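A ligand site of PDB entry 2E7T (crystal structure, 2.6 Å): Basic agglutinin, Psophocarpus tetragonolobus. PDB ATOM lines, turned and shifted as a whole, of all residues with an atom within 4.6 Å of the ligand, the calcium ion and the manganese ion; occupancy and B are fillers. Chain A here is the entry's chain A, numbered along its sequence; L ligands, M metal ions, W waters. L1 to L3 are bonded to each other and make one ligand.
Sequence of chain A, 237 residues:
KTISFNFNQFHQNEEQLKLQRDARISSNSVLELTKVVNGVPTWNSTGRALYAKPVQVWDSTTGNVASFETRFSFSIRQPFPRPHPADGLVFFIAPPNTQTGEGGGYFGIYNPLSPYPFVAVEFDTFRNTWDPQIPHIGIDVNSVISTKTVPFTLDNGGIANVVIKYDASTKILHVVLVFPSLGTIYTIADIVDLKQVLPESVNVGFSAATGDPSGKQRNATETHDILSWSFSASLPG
Of the 25 residues printed, 4 come within 4 Å of the manganese ion. The nearest printed residue that does not touch the manganese ion is Ser 146 (4.2 Å).
Merely in contact with the ligand: Gly 104, Tyr 106, Trp 130, Gly 211, Gly 215 and Ala 220. Hydrophobic or aromatic side chains within 4 Å of the ligand: His 84, Tyr 106, Phe 126, Trp 130 and Ala 220.
The calcium ion is bound by the side-chain amide oxygen (OD1) of Asn 128 (2.4 Å), the side-chain carboxylate (OD1) of Asp 124 (2.5 Å), the backbone carbonyl oxygen (O) of Phe 126 (2.6 Å), the side-chain carboxylate (OD2) of Asp 124 (2.6 Å), the side-chain carboxylate (OD2) of Asp 131 (2.7 Å) and water W1 (2.7 Å). The calcium ion has six donor atoms within binding distance.
The side-chain carboxylate (OD1) of Asp 131 lies close to the indole nitrogen (NE1) of Trp 130 (3.5 Å). OG of Ser 214 lies within hydrogen-bond range of OD2 of Asp 212. OD2 of Asp 87 lies within hydrogen-bond range of N of Gly 105 (3.5 Å). N of Gly 211 sits at hydrogen-bond distance from O of Ala 220, at 2.6 Å.
Water W1 lies within hydrogen-bond range of the backbone carbonyl oxygen (O) of Gly 105 (2.7 Å) and the indole nitrogen (NE1) of Trp 130 (3.1 Å). Water W3 lies within hydrogen-bond range of O of Asp 212 (2.7 Å), O of Gln 217 (2.9 Å) and O4 of LG3 L3 (3.3 Å).
Four residues have an atom within 4 Å of the calcium ion: Asp 124, Phe 126, Asn 128 and Asp 131.
O2 of LG3 L3 lies within hydrogen-bond range of OD2 of Asp 87. The backbone NH of Asp 212 sits at hydrogen-bond distance from an oxygen (O3) of LG3 L3 (2.8 Å). The side-chain amide nitrogen (ND2) of Asn 128 lies within hydrogen-bond range of an oxygen (O2) of LG3 L3. NZ of Lys 216 is in hydrogen-bond range of O3 of LIG L1, 3.3 Å away. An oxygen (O2) of LG3 L3 lies within hydrogen-bond range of the backbone NH (N) of Gly 105 (2.6 Å). O3 of LIG L1 is in hydrogen-bond range of O of Ser 214 (2.7 Å). NE2 of His 84 is in hydrogen-bond range of O4 of LG3 L3. O1 of LG2 L2 is in hydrogen-bond range of OG of Ser 214.
The manganese ion is bound by the side-chain carboxylate of Glu 122 (2.2 Å), the side-chain carboxylate of Asp 124 (2.3 Å), the side-chain carboxylate of Asp 131 (2.3 Å), water W2 (2.4 Å) and a ring nitrogen (NE2) of His 136 (2.6 Å). The manganese ion has five donor atoms within binding distance.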
ATOM      1  N   HIS A  84       8.739 -21.601  26.706  1.00  0.00           N
ATOM      2  CA  HIS A  84       9.634 -20.615  26.135  1.00  0.00           C
ATOM      3  C   HIS A  84       9.676 -19.275  26.899  1.00  0.00           C
ATOM      4  O   HIS A  84       8.641 -18.678  27.195  1.00  0.00           O
ATOM      5  CB  HIS A  84       9.225 -20.331  24.696  1.00  0.00           C
ATOM      6  CG  HIS A  84       7.768 -20.012  24.548  1.00  0.00           C
ATOM      7  ND1 HIS A  84       6.837 -20.955  24.165  1.00  0.00           N
ATOM      8  CD2 HIS A  84       7.077 -18.866  24.768  1.00  0.00           C
ATOM      9  CE1 HIS A  84       5.631 -20.401  24.155  1.00  0.00           C
ATOM     10  NE2 HIS A  84       5.757 -19.144  24.518  1.00  0.00           N
ATOM     11  N   ALA A  86      10.361 -15.234  27.619  1.00  0.00           N
ATOM     12  CA  ALA A  86      10.029 -14.018  26.863  1.00  0.00           C
ATOM     13  C   ALA A  86      10.144 -12.839  27.809  1.00  0.00           C
ATOM     14  O   ALA A  86       9.933 -13.002  29.012  1.00  0.00           O
ATOM     15  CB  ALA A  86       8.625 -14.109  26.323  1.00  0.00           C
ATOM     16  N   ASP A  87      10.444 -11.650  27.286  1.00  0.00           N
ATOM     17  CA  ASP A  87      10.666 -11.444  25.861  1.00  0.00           C
ATOM     18  C   ASP A  87      12.061 -10.902  25.590  1.00  0.00           C
ATOM     19  O   ASP A  87      12.639 -11.157  24.521  1.00  0.00           O
ATOM     20  CB  ASP A  87       9.634 -10.468  25.278  1.00  0.00           C
ATOM     21  CG  ASP A  87       8.342 -11.165  24.853  1.00  0.00           C
ATOM     22  OD1 ASP A  87       7.399 -11.281  25.685  1.00  0.00           O
ATOM     23  OD2 ASP A  87       8.262 -11.602  23.677  1.00  0.00           O
ATOM     24  N   GLY A 103       3.774  -4.190  25.327  1.00  0.00           N
ATOM     25  CA  GLY A 103       4.711  -5.119  25.903  1.00  0.00           C
ATOM     26  C   GLY A 103       5.053  -6.246  24.943  1.00  0.00           C
ATOM     27  O   GLY A 103       5.139  -6.016  23.743  1.00  0.00           O
ATOM     28  N   GLY A 104       5.239  -7.443  25.480  1.00  0.00           N
ATOM     29  CA  GLY A 104       5.580  -8.573  24.651  1.00  0.00           C
ATOM     30  C   GLY A 104       6.782  -8.334  23.755  1.00  0.00           C
ATOM     31  O   GLY A 104       7.797  -7.794  24.201  1.00  0.00           O
ATOM     32  N   GLY A 105       6.668  -8.741  22.497  1.00  0.00           N
ATOM     33  CA  GLY A 105       7.756  -8.588  21.547  1.00  0.00           C
ATOM     34  C   GLY A 105       8.042  -7.154  21.173  1.00  0.00           C
ATOM     35  O   GLY A 105       8.955  -6.902  20.369  1.00  0.00           O
ATOM     36  N   TYR A 106       7.284  -6.206  21.725  1.00  0.00           N
ATOM     37  CA  TYR A 106       7.531  -4.804  21.446  1.00  0.00           C
ATOM     38  C   TYR A 106       8.396  -4.157  22.527  1.00  0.00           C
ATOM     39  O   TYR A 106       8.692  -2.955  22.486  1.00  0.00           O
ATOM     40  CB  TYR A 106       6.219  -4.074  21.278  1.00  0.00           C
ATOM     41  CG  TYR A 106       5.494  -4.526  20.037  1.00  0.00           C
ATOM     42  CD1 TYR A 106       5.986  -4.230  18.778  1.00  0.00           C
ATOM     43  CD2 TYR A 106       4.328  -5.278  20.125  1.00  0.00           C
ATOM     44  CE1 TYR A 106       5.344  -4.670  17.607  1.00  0.00           C
ATOM     45  CE2 TYR A 106       3.670  -5.741  18.971  1.00  0.00           C
ATOM     46  CZ  TYR A 106       4.193  -5.426  17.720  1.00  0.00           C
ATOM     47  OH  TYR A 106       3.544  -5.887  16.577  1.00  0.00           O
ATOM     48  N   PHE A 107       8.805  -4.981  23.490  1.00  0.00           N
ATOM     49  CA  PHE A 107       9.691  -4.559  24.588  1.00  0.00           C
ATOM     50  C   PHE A 107       9.242  -3.343  25.392  1.00  0.00           C
ATOM     51  O   PHE A 107       9.934  -2.927  26.297  1.00  0.00           O
ATOM     52  CB  PHE A 107      11.104  -4.296  24.052  1.00  0.00           C
ATOM     53  CG  PHE A 107      11.686  -5.431  23.241  1.00  0.00           C
ATOM     54  CD1 PHE A 107      11.962  -6.657  23.832  1.00  0.00           C
ATOM     55  CD2 PHE A 107      11.973  -5.263  21.893  1.00  0.00           C
ATOM     56  CE1 PHE A 107      12.543  -7.696  23.101  1.00  0.00           C
ATOM     57  CE2 PHE A 107      12.546  -6.291  21.157  1.00  0.00           C
ATOM     58  CZ  PHE A 107      12.841  -7.516  21.760  1.00  0.00           C
ATOM     59  N   GLU A 122      18.615  -4.481  21.073  1.00  0.00           N
ATOM     60  CA  GLU A 122      17.851  -5.488  21.764  1.00  0.00           C
ATOM     61  C   GLU A 122      18.591  -6.786  22.077  1.00  0.00           C
ATOM     62  O   GLU A 122      19.520  -7.192  21.378  1.00  0.00           O
ATOM     63  CB  GLU A 122      16.611  -5.829  20.963  1.00  0.00           C
ATOM     64  CG  GLU A 122      16.944  -6.495  19.642  1.00  0.00           C
ATOM     65  CD  GLU A 122      15.730  -7.087  18.935  1.00  0.00           C
ATOM     66  OE1 GLU A 122      14.792  -6.328  18.623  1.00  0.00           O
ATOM     67  OE2 GLU A 122      15.731  -8.323  18.686  1.00  0.00           O
ATOM     68  N   ASP A 124      17.008 -10.020  22.493  1.00  0.00           N
ATOM     69  CA  ASP A 124      15.775 -10.733  22.255  1.00  0.00           C
ATOM     70  C   ASP A 124      15.835 -12.176  22.628  1.00  0.00           C
ATOM     71  O   ASP A 124      16.704 -12.898  22.127  1.00  0.00           O
ATOM     72  CB  ASP A 124      15.436 -10.597  20.776  1.00  0.00           C
ATOM     73  CG  ASP A 124      13.960 -10.770  20.499  1.00  0.00           C
ATOM     74  OD1 ASP A 124      13.291 -11.496  21.260  1.00  0.00           O
ATOM     75  OD2 ASP A 124      13.473 -10.171  19.531  1.00  0.00           O
ATOM     76  N   PHE A 126      12.686 -14.257  22.808  1.00  0.00           N
ATOM     77  CA  PHE A 126      11.515 -14.957  22.322  1.00  0.00           C
ATOM     78  C   PHE A 126      11.433 -14.731  20.834  1.00  0.00           C
ATOM     79  O   PHE A 126      11.655 -13.615  20.364  1.00  0.00           O
ATOM     80  CB  PHE A 126      10.244 -14.410  22.970  1.00  0.00           C
ATOM     81  CG  PHE A 126       8.999 -14.999  22.398  1.00  0.00           C
ATOM     82  CD1 PHE A 126       8.546 -16.247  22.809  1.00  0.00           C
ATOM     83  CD2 PHE A 126       8.270 -14.302  21.429  1.00  0.00           C
ATOM     84  CE1 PHE A 126       7.380 -16.803  22.276  1.00  0.00           C
ATOM     85  CE2 PHE A 126       7.107 -14.840  20.890  1.00  0.00           C
ATOM     86  CZ  PHE A 126       6.652 -16.097  21.304  1.00  0.00           C
ATOM     87  N   ASN A 128       9.470 -14.050  17.676  1.00  0.00           N
ATOM     88  CA  ASN A 128       8.205 -13.654  17.084  1.00  0.00           C
ATOM     89  C   ASN A 128       8.229 -13.978  15.602  1.00  0.00           C
ATOM     90  O   ASN A 128       9.246 -14.428  15.083  1.00  0.00           O
ATOM     91  CB  ASN A 128       7.950 -12.155  17.274  1.00  0.00           C
ATOM     92  CG  ASN A 128       7.796 -11.778  18.720  1.00  0.00           C
ATOM     93  OD1 ASN A 128       8.779 -11.650  19.438  1.00  0.00           O
ATOM     94  ND2 ASN A 128       6.573 -11.613  19.159  1.00  0.00           N
ATOM     95  N   TRP A 130       8.474 -12.143  13.164  1.00  0.00           N
ATOM     96  CA  TRP A 130       9.479 -11.330  12.480  1.00  0.00           C
ATOM     97  C   TRP A 130      10.923 -11.565  12.897  1.00  0.00           C
ATOM     98  O   TRP A 130      11.820 -10.889  12.397  1.00  0.00           O
ATOM     99  CB  TRP A 130       9.136  -9.863  12.684  1.00  0.00           C
ATOM    100  CG  TRP A 130       9.203  -9.445  14.117  1.00  0.00           C
ATOM    101  CD1 TRP A 130      10.335  -9.223  14.867  1.00  0.00           C
ATOM    102  CD2 TRP A 130       8.091  -9.218  14.998  1.00  0.00           C
ATOM    103  NE1 TRP A 130       9.989  -8.873  16.151  1.00  0.00           N
ATOM    104  CE2 TRP A 130       8.626  -8.865  16.258  1.00  0.00           C
ATOM    105  CE3 TRP A 130       6.691  -9.270  14.843  1.00  0.00           C
ATOM    106  CZ2 TRP A 130       7.816  -8.556  17.356  1.00  0.00           C
ATOM    107  CZ3 TRP A 130       5.889  -8.972  15.946  1.00  0.00           C
ATOM    108  CH2 TRP A 130       6.449  -8.623  17.178  1.00  0.00           C
ATOM    109  N   ASP A 131      11.143 -12.538  13.780  1.00  0.00           N
ATOM    110  CA  ASP A 131      12.468 -12.862  14.306  1.00  0.00           C
ATOM    111  C   ASP A 131      13.216 -14.045  13.761  1.00  0.00           C
ATOM    112  O   ASP A 131      12.630 -15.014  13.307  1.00  0.00           O
ATOM    113  CB  ASP A 131      12.406 -13.164  15.809  1.00  0.00           C
ATOM    114  CG  ASP A 131      12.247 -11.942  16.653  1.00  0.00           C
ATOM    115  OD1 ASP A 131      12.821 -10.880  16.298  1.00  0.00           O
ATOM    116  OD2 ASP A 131      11.562 -12.089  17.699  1.00  0.00           O
ATOM    117  N   HIS A 136      19.196 -13.368  20.336  1.00  0.00           N
ATOM    118  CA  HIS A 136      20.027 -12.642  19.397  1.00  0.00           C
ATOM    119  C   HIS A 136      20.133 -11.174  19.791  1.00  0.00           C
ATOM    120  O   HIS A 136      19.304 -10.651  20.530  1.00  0.00           O
ATOM    121  CB  HIS A 136      19.499 -12.752  17.952  1.00  0.00           C
ATOM    122  CG  HIS A 136      18.074 -12.302  17.765  1.00  0.00           C
ATOM    123  ND1 HIS A 136      17.020 -13.191  17.748  1.00  0.00           N
ATOM    124  CD2 HIS A 136      17.547 -11.075  17.537  1.00  0.00           C
ATOM    125  CE1 HIS A 136      15.894 -12.519  17.516  1.00  0.00           C
ATOM    126  NE2 HIS A 136      16.184 -11.245  17.379  1.00  0.00           N
ATOM    127  N   VAL A 144      10.944  -3.001  15.684  1.00  0.00           N
ATOM    128  CA  VAL A 144      11.559  -4.167  16.310  1.00  0.00           C
ATOM    129  C   VAL A 144      11.982  -5.158  15.260  1.00  0.00           C
ATOM    130  O   VAL A 144      12.367  -6.269  15.578  1.00  0.00           O
ATOM    131  CB  VAL A 144      10.624  -4.855  17.298  1.00  0.00           C
ATOM    132  CG1 VAL A 144      10.321  -3.897  18.460  1.00  0.00           C
ATOM    133  CG2 VAL A 144       9.352  -5.251  16.591  1.00  0.00           C
ATOM    134  N   SER A 146      14.684  -5.718  13.366  1.00  0.00           N
ATOM    135  CA  SER A 146      16.097  -5.338  13.304  1.00  0.00           C
ATOM    136  C   SER A 146      16.691  -5.207  11.918  1.00  0.00           C
ATOM    137  O   SER A 146      16.349  -5.953  10.999  1.00  0.00           O
ATOM    138  CB  SER A 146      16.929  -6.366  14.081  1.00  0.00           C
ATOM    139  OG  SER A 146      16.384  -6.568  15.361  1.00  0.00           O
ATOM    140  N   THR A 210       7.934  -9.217  29.735  1.00  0.00           N
ATOM    141  CA  THR A 210       7.780 -10.670  29.839  1.00  0.00           C
ATOM    142  C   THR A 210       6.588 -11.102  28.993  1.00  0.00           C
ATOM    143  O   THR A 210       5.884 -10.258  28.422  1.00  0.00           O
ATOM    144  CB  THR A 210       7.584 -11.114  31.308  1.00  0.00           C
ATOM    145  OG1 THR A 210       6.543 -10.334  31.908  1.00  0.00           O
ATOM    146  CG2 THR A 210       8.872 -10.911  32.083  1.00  0.00           C
ATOM    147  N   GLY A 211       6.360 -12.407  28.910  1.00  0.00           N
ATOM    148  CA  GLY A 211       5.270 -12.940  28.105  1.00  0.00           C
ATOM    149  C   GLY A 211       3.941 -12.213  28.175  1.00  0.00           C
ATOM    150  O   GLY A 211       3.449 -11.917  29.248  1.00  0.00           O
ATOM    151  N   ASP A 212       3.376 -11.926  27.010  1.00  0.00           N
ATOM    152  CA  ASP A 212       2.080 -11.254  26.953  1.00  0.00           C
ATOM    153  C   ASP A 212       0.985 -12.308  27.194  1.00  0.00           C
ATOM    154  O   ASP A 212       1.092 -13.449  26.734  1.00  0.00           O
ATOM    155  CB  ASP A 212       1.867 -10.609  25.586  1.00  0.00           C
ATOM    156  CG  ASP A 212       0.521  -9.900  25.487  1.00  0.00           C
ATOM    157  OD1 ASP A 212       0.305  -8.930  26.242  1.00  0.00           O
ATOM    158  OD2 ASP A 212      -0.322 -10.337  24.682  1.00  0.00           O
ATOM    159  N   SER A 214      -1.788 -12.867  25.857  1.00  0.00           N
ATOM    160  CA  SER A 214      -2.310 -13.422  24.614  1.00  0.00           C
ATOM    161  C   SER A 214      -1.684 -14.756  24.268  1.00  0.00           C
ATOM    162  O   SER A 214      -2.281 -15.559  23.562  1.00  0.00           O
ATOM    163  CB  SER A 214      -2.089 -12.447  23.464  1.00  0.00           C
ATOM    164  OG  SER A 214      -0.727 -12.385  23.090  1.00  0.00           O
ATOM    165  N   GLY A 215      -0.465 -14.985  24.765  1.00  0.00           N
ATOM    166  CA  GLY A 215       0.233 -16.229  24.489  1.00  0.00           C
ATOM    167  C   GLY A 215      -0.258 -17.389  25.337  1.00  0.00           C
ATOM    168  O   GLY A 215       0.095 -18.553  25.108  1.00  0.00           O
ATOM    169  N   LYS A 216      -1.072 -17.062  26.340  1.00  0.00           N
ATOM    170  CA  LYS A 216      -1.654 -18.068  27.235  1.00  0.00           C
ATOM    171  C   LYS A 216      -0.616 -18.954  27.913  1.00  0.00           C
ATOM    172  O   LYS A 216      -0.857 -20.155  28.123  1.00  0.00           O
ATOM    173  CB  LYS A 216      -2.636 -18.948  26.453  1.00  0.00           C
ATOM    174  CG  LYS A 216      -3.832 -18.195  25.833  1.00  0.00           C
ATOM    175  CD  LYS A 216      -4.614 -19.097  24.864  1.00  0.00           C
ATOM    176  CE  LYS A 216      -5.939 -18.489  24.429  1.00  0.00           C
ATOM    177  NZ  LYS A 216      -5.782 -17.189  23.672  1.00  0.00           N
ATOM    178  N   GLN A 217       0.545 -18.378  28.242  1.00  0.00           N
ATOM    179  CA  GLN A 217       1.611 -19.131  28.913  1.00  0.00           C
ATOM    180  C   GLN A 217       2.225 -18.312  30.037  1.00  0.00           C
ATOM    181  O   GLN A 217       2.876 -17.293  29.806  1.00  0.00           O
ATOM    182  CB  GLN A 217       2.702 -19.520  27.911  1.00  0.00           C
ATOM    183  CG  GLN A 217       2.231 -20.448  26.825  1.00  0.00           C
ATOM    184  CD  GLN A 217       2.051 -21.885  27.299  1.00  0.00           C
ATOM    185  OE1 GLN A 217       1.460 -22.707  26.601  1.00  0.00           O
ATOM    186  NE2 GLN A 217       2.581 -22.192  28.478  1.00  0.00           N
ATOM    187  N   ALA A 220       6.092 -18.053  30.098  1.00  0.00           N
ATOM    188  CA  ALA A 220       6.768 -17.183  29.149  1.00  0.00           C
ATOM    189  C   ALA A 220       7.314 -15.982  29.906  1.00  0.00           C
ATOM    190  O   ALA A 220       6.824 -14.853  29.753  1.00  0.00           O
ATOM    191  CB  ALA A 220       5.789 -16.709  28.102  1.00  0.00           C
HETATM  192  C1  LIG L   1      -4.075 -18.131  18.126  1.00  0.00           C
HETATM  193  C2  LIG L   1      -4.153 -18.135  19.637  1.00  0.00           C
HETATM  194  C3  LIG L   1      -3.231 -17.092  20.217  1.00  0.00           C
HETATM  195  C4  LIG L   1      -1.804 -17.210  19.685  1.00  0.00           C
HETATM  196  C5  LIG L   1      -1.814 -17.328  18.127  1.00  0.00           C
HETATM  197  C6  LIG L   1      -0.450 -17.666  17.502  1.00  0.00           C
HETATM  198  O1  LIG L   1      -4.471 -16.904  17.652  1.00  0.00           O
HETATM  199  O2  LIG L   1      -5.481 -17.862  20.052  1.00  0.00           O
HETATM  200  O3  LIG L   1      -3.209 -17.254  21.618  1.00  0.00           O
HETATM  201  O4  LIG L   1      -1.061 -16.055  20.134  1.00  0.00           O
HETATM  202  O5  LIG L   1      -2.721 -18.366  17.709  1.00  0.00           O
HETATM  203  O6  LIG L   1      -0.565 -18.049  16.138  1.00  0.00           O
HETATM  204  C1  LG2 L   2       0.270 -15.964  19.789  1.00  0.00           C
HETATM  205  C2  LG2 L   2       1.014 -14.978  20.676  1.00  0.00           C
HETATM  206  C3  LG2 L   2       2.464 -14.971  20.225  1.00  0.00           C
HETATM  207  C4  LG2 L   2       3.027 -16.365  20.233  1.00  0.00           C
HETATM  208  C5  LG2 L   2       2.181 -17.295  19.388  1.00  0.00           C
HETATM  209  C6  LG2 L   2       2.658 -18.726  19.454  1.00  0.00           C
HETATM  210  O1  LG2 L   2       0.441 -13.691  20.526  1.00  0.00           O
HETATM  211  O2  LG2 L   2       3.319 -14.131  21.010  1.00  0.00           O
HETATM  212  O3  LG2 L   2       3.033 -16.834  21.561  1.00  0.00           O
HETATM  213  O4  LG2 L   2       0.840 -17.255  19.896  1.00  0.00           O
HETATM  214  O5  LG2 L   2       1.582 -19.637  19.368  1.00  0.00           O
HETATM  215  O1  LG3 L   3       3.052 -14.057  23.314  1.00  0.00           O
HETATM  216  C1  LG3 L   3       2.873 -13.362  22.092  1.00  0.00           C
HETATM  217  C2  LG3 L   3       3.702 -12.061  22.113  1.00  0.00           C
HETATM  218  N1  LG3 L   3       3.539 -11.348  20.864  1.00  0.00           N
HETATM  219  C3  LG3 L   3       5.172 -12.417  22.343  1.00  0.00           C
HETATM  220  O2  LG3 L   3       5.995 -11.285  22.399  1.00  0.00           O
HETATM  221  C4  LG3 L   3       5.310 -13.215  23.613  1.00  0.00           C
HETATM  222  O3  LG3 L   3       4.979 -12.406  24.713  1.00  0.00           O
HETATM  223  C5  LG3 L   3       4.418 -14.434  23.606  1.00  0.00           C
HETATM  224  C6  LG3 L   3       4.409 -15.059  24.974  1.00  0.00           C
HETATM  225  O4  LG3 L   3       4.128 -16.433  24.913  1.00  0.00           O
HETATM  226  C7  LG3 L   3       3.365 -10.040  20.848  1.00  0.00           C
HETATM  227  O5  LG3 L   3       3.279  -9.373  21.837  1.00  0.00           O
HETATM  228  C8  LG3 L   3       3.291  -9.403  19.498  1.00  0.00           C
HETATM  229 CA    CA M   1      11.056 -11.082  20.110  1.00  0.00          CA
HETATM  230 MN    MN M   2      14.267  -9.514  17.488  1.00  0.00          MN
HETATM  231  O   HOH W   1      10.697  -8.561  19.117  1.00  0.00           O
HETATM  232  O   HOH W   2      15.001  -8.912  15.331  1.00  0.00           O
HETATM  233  O   HOH W   3       2.081 -15.916  27.406  1.00  0.00           O
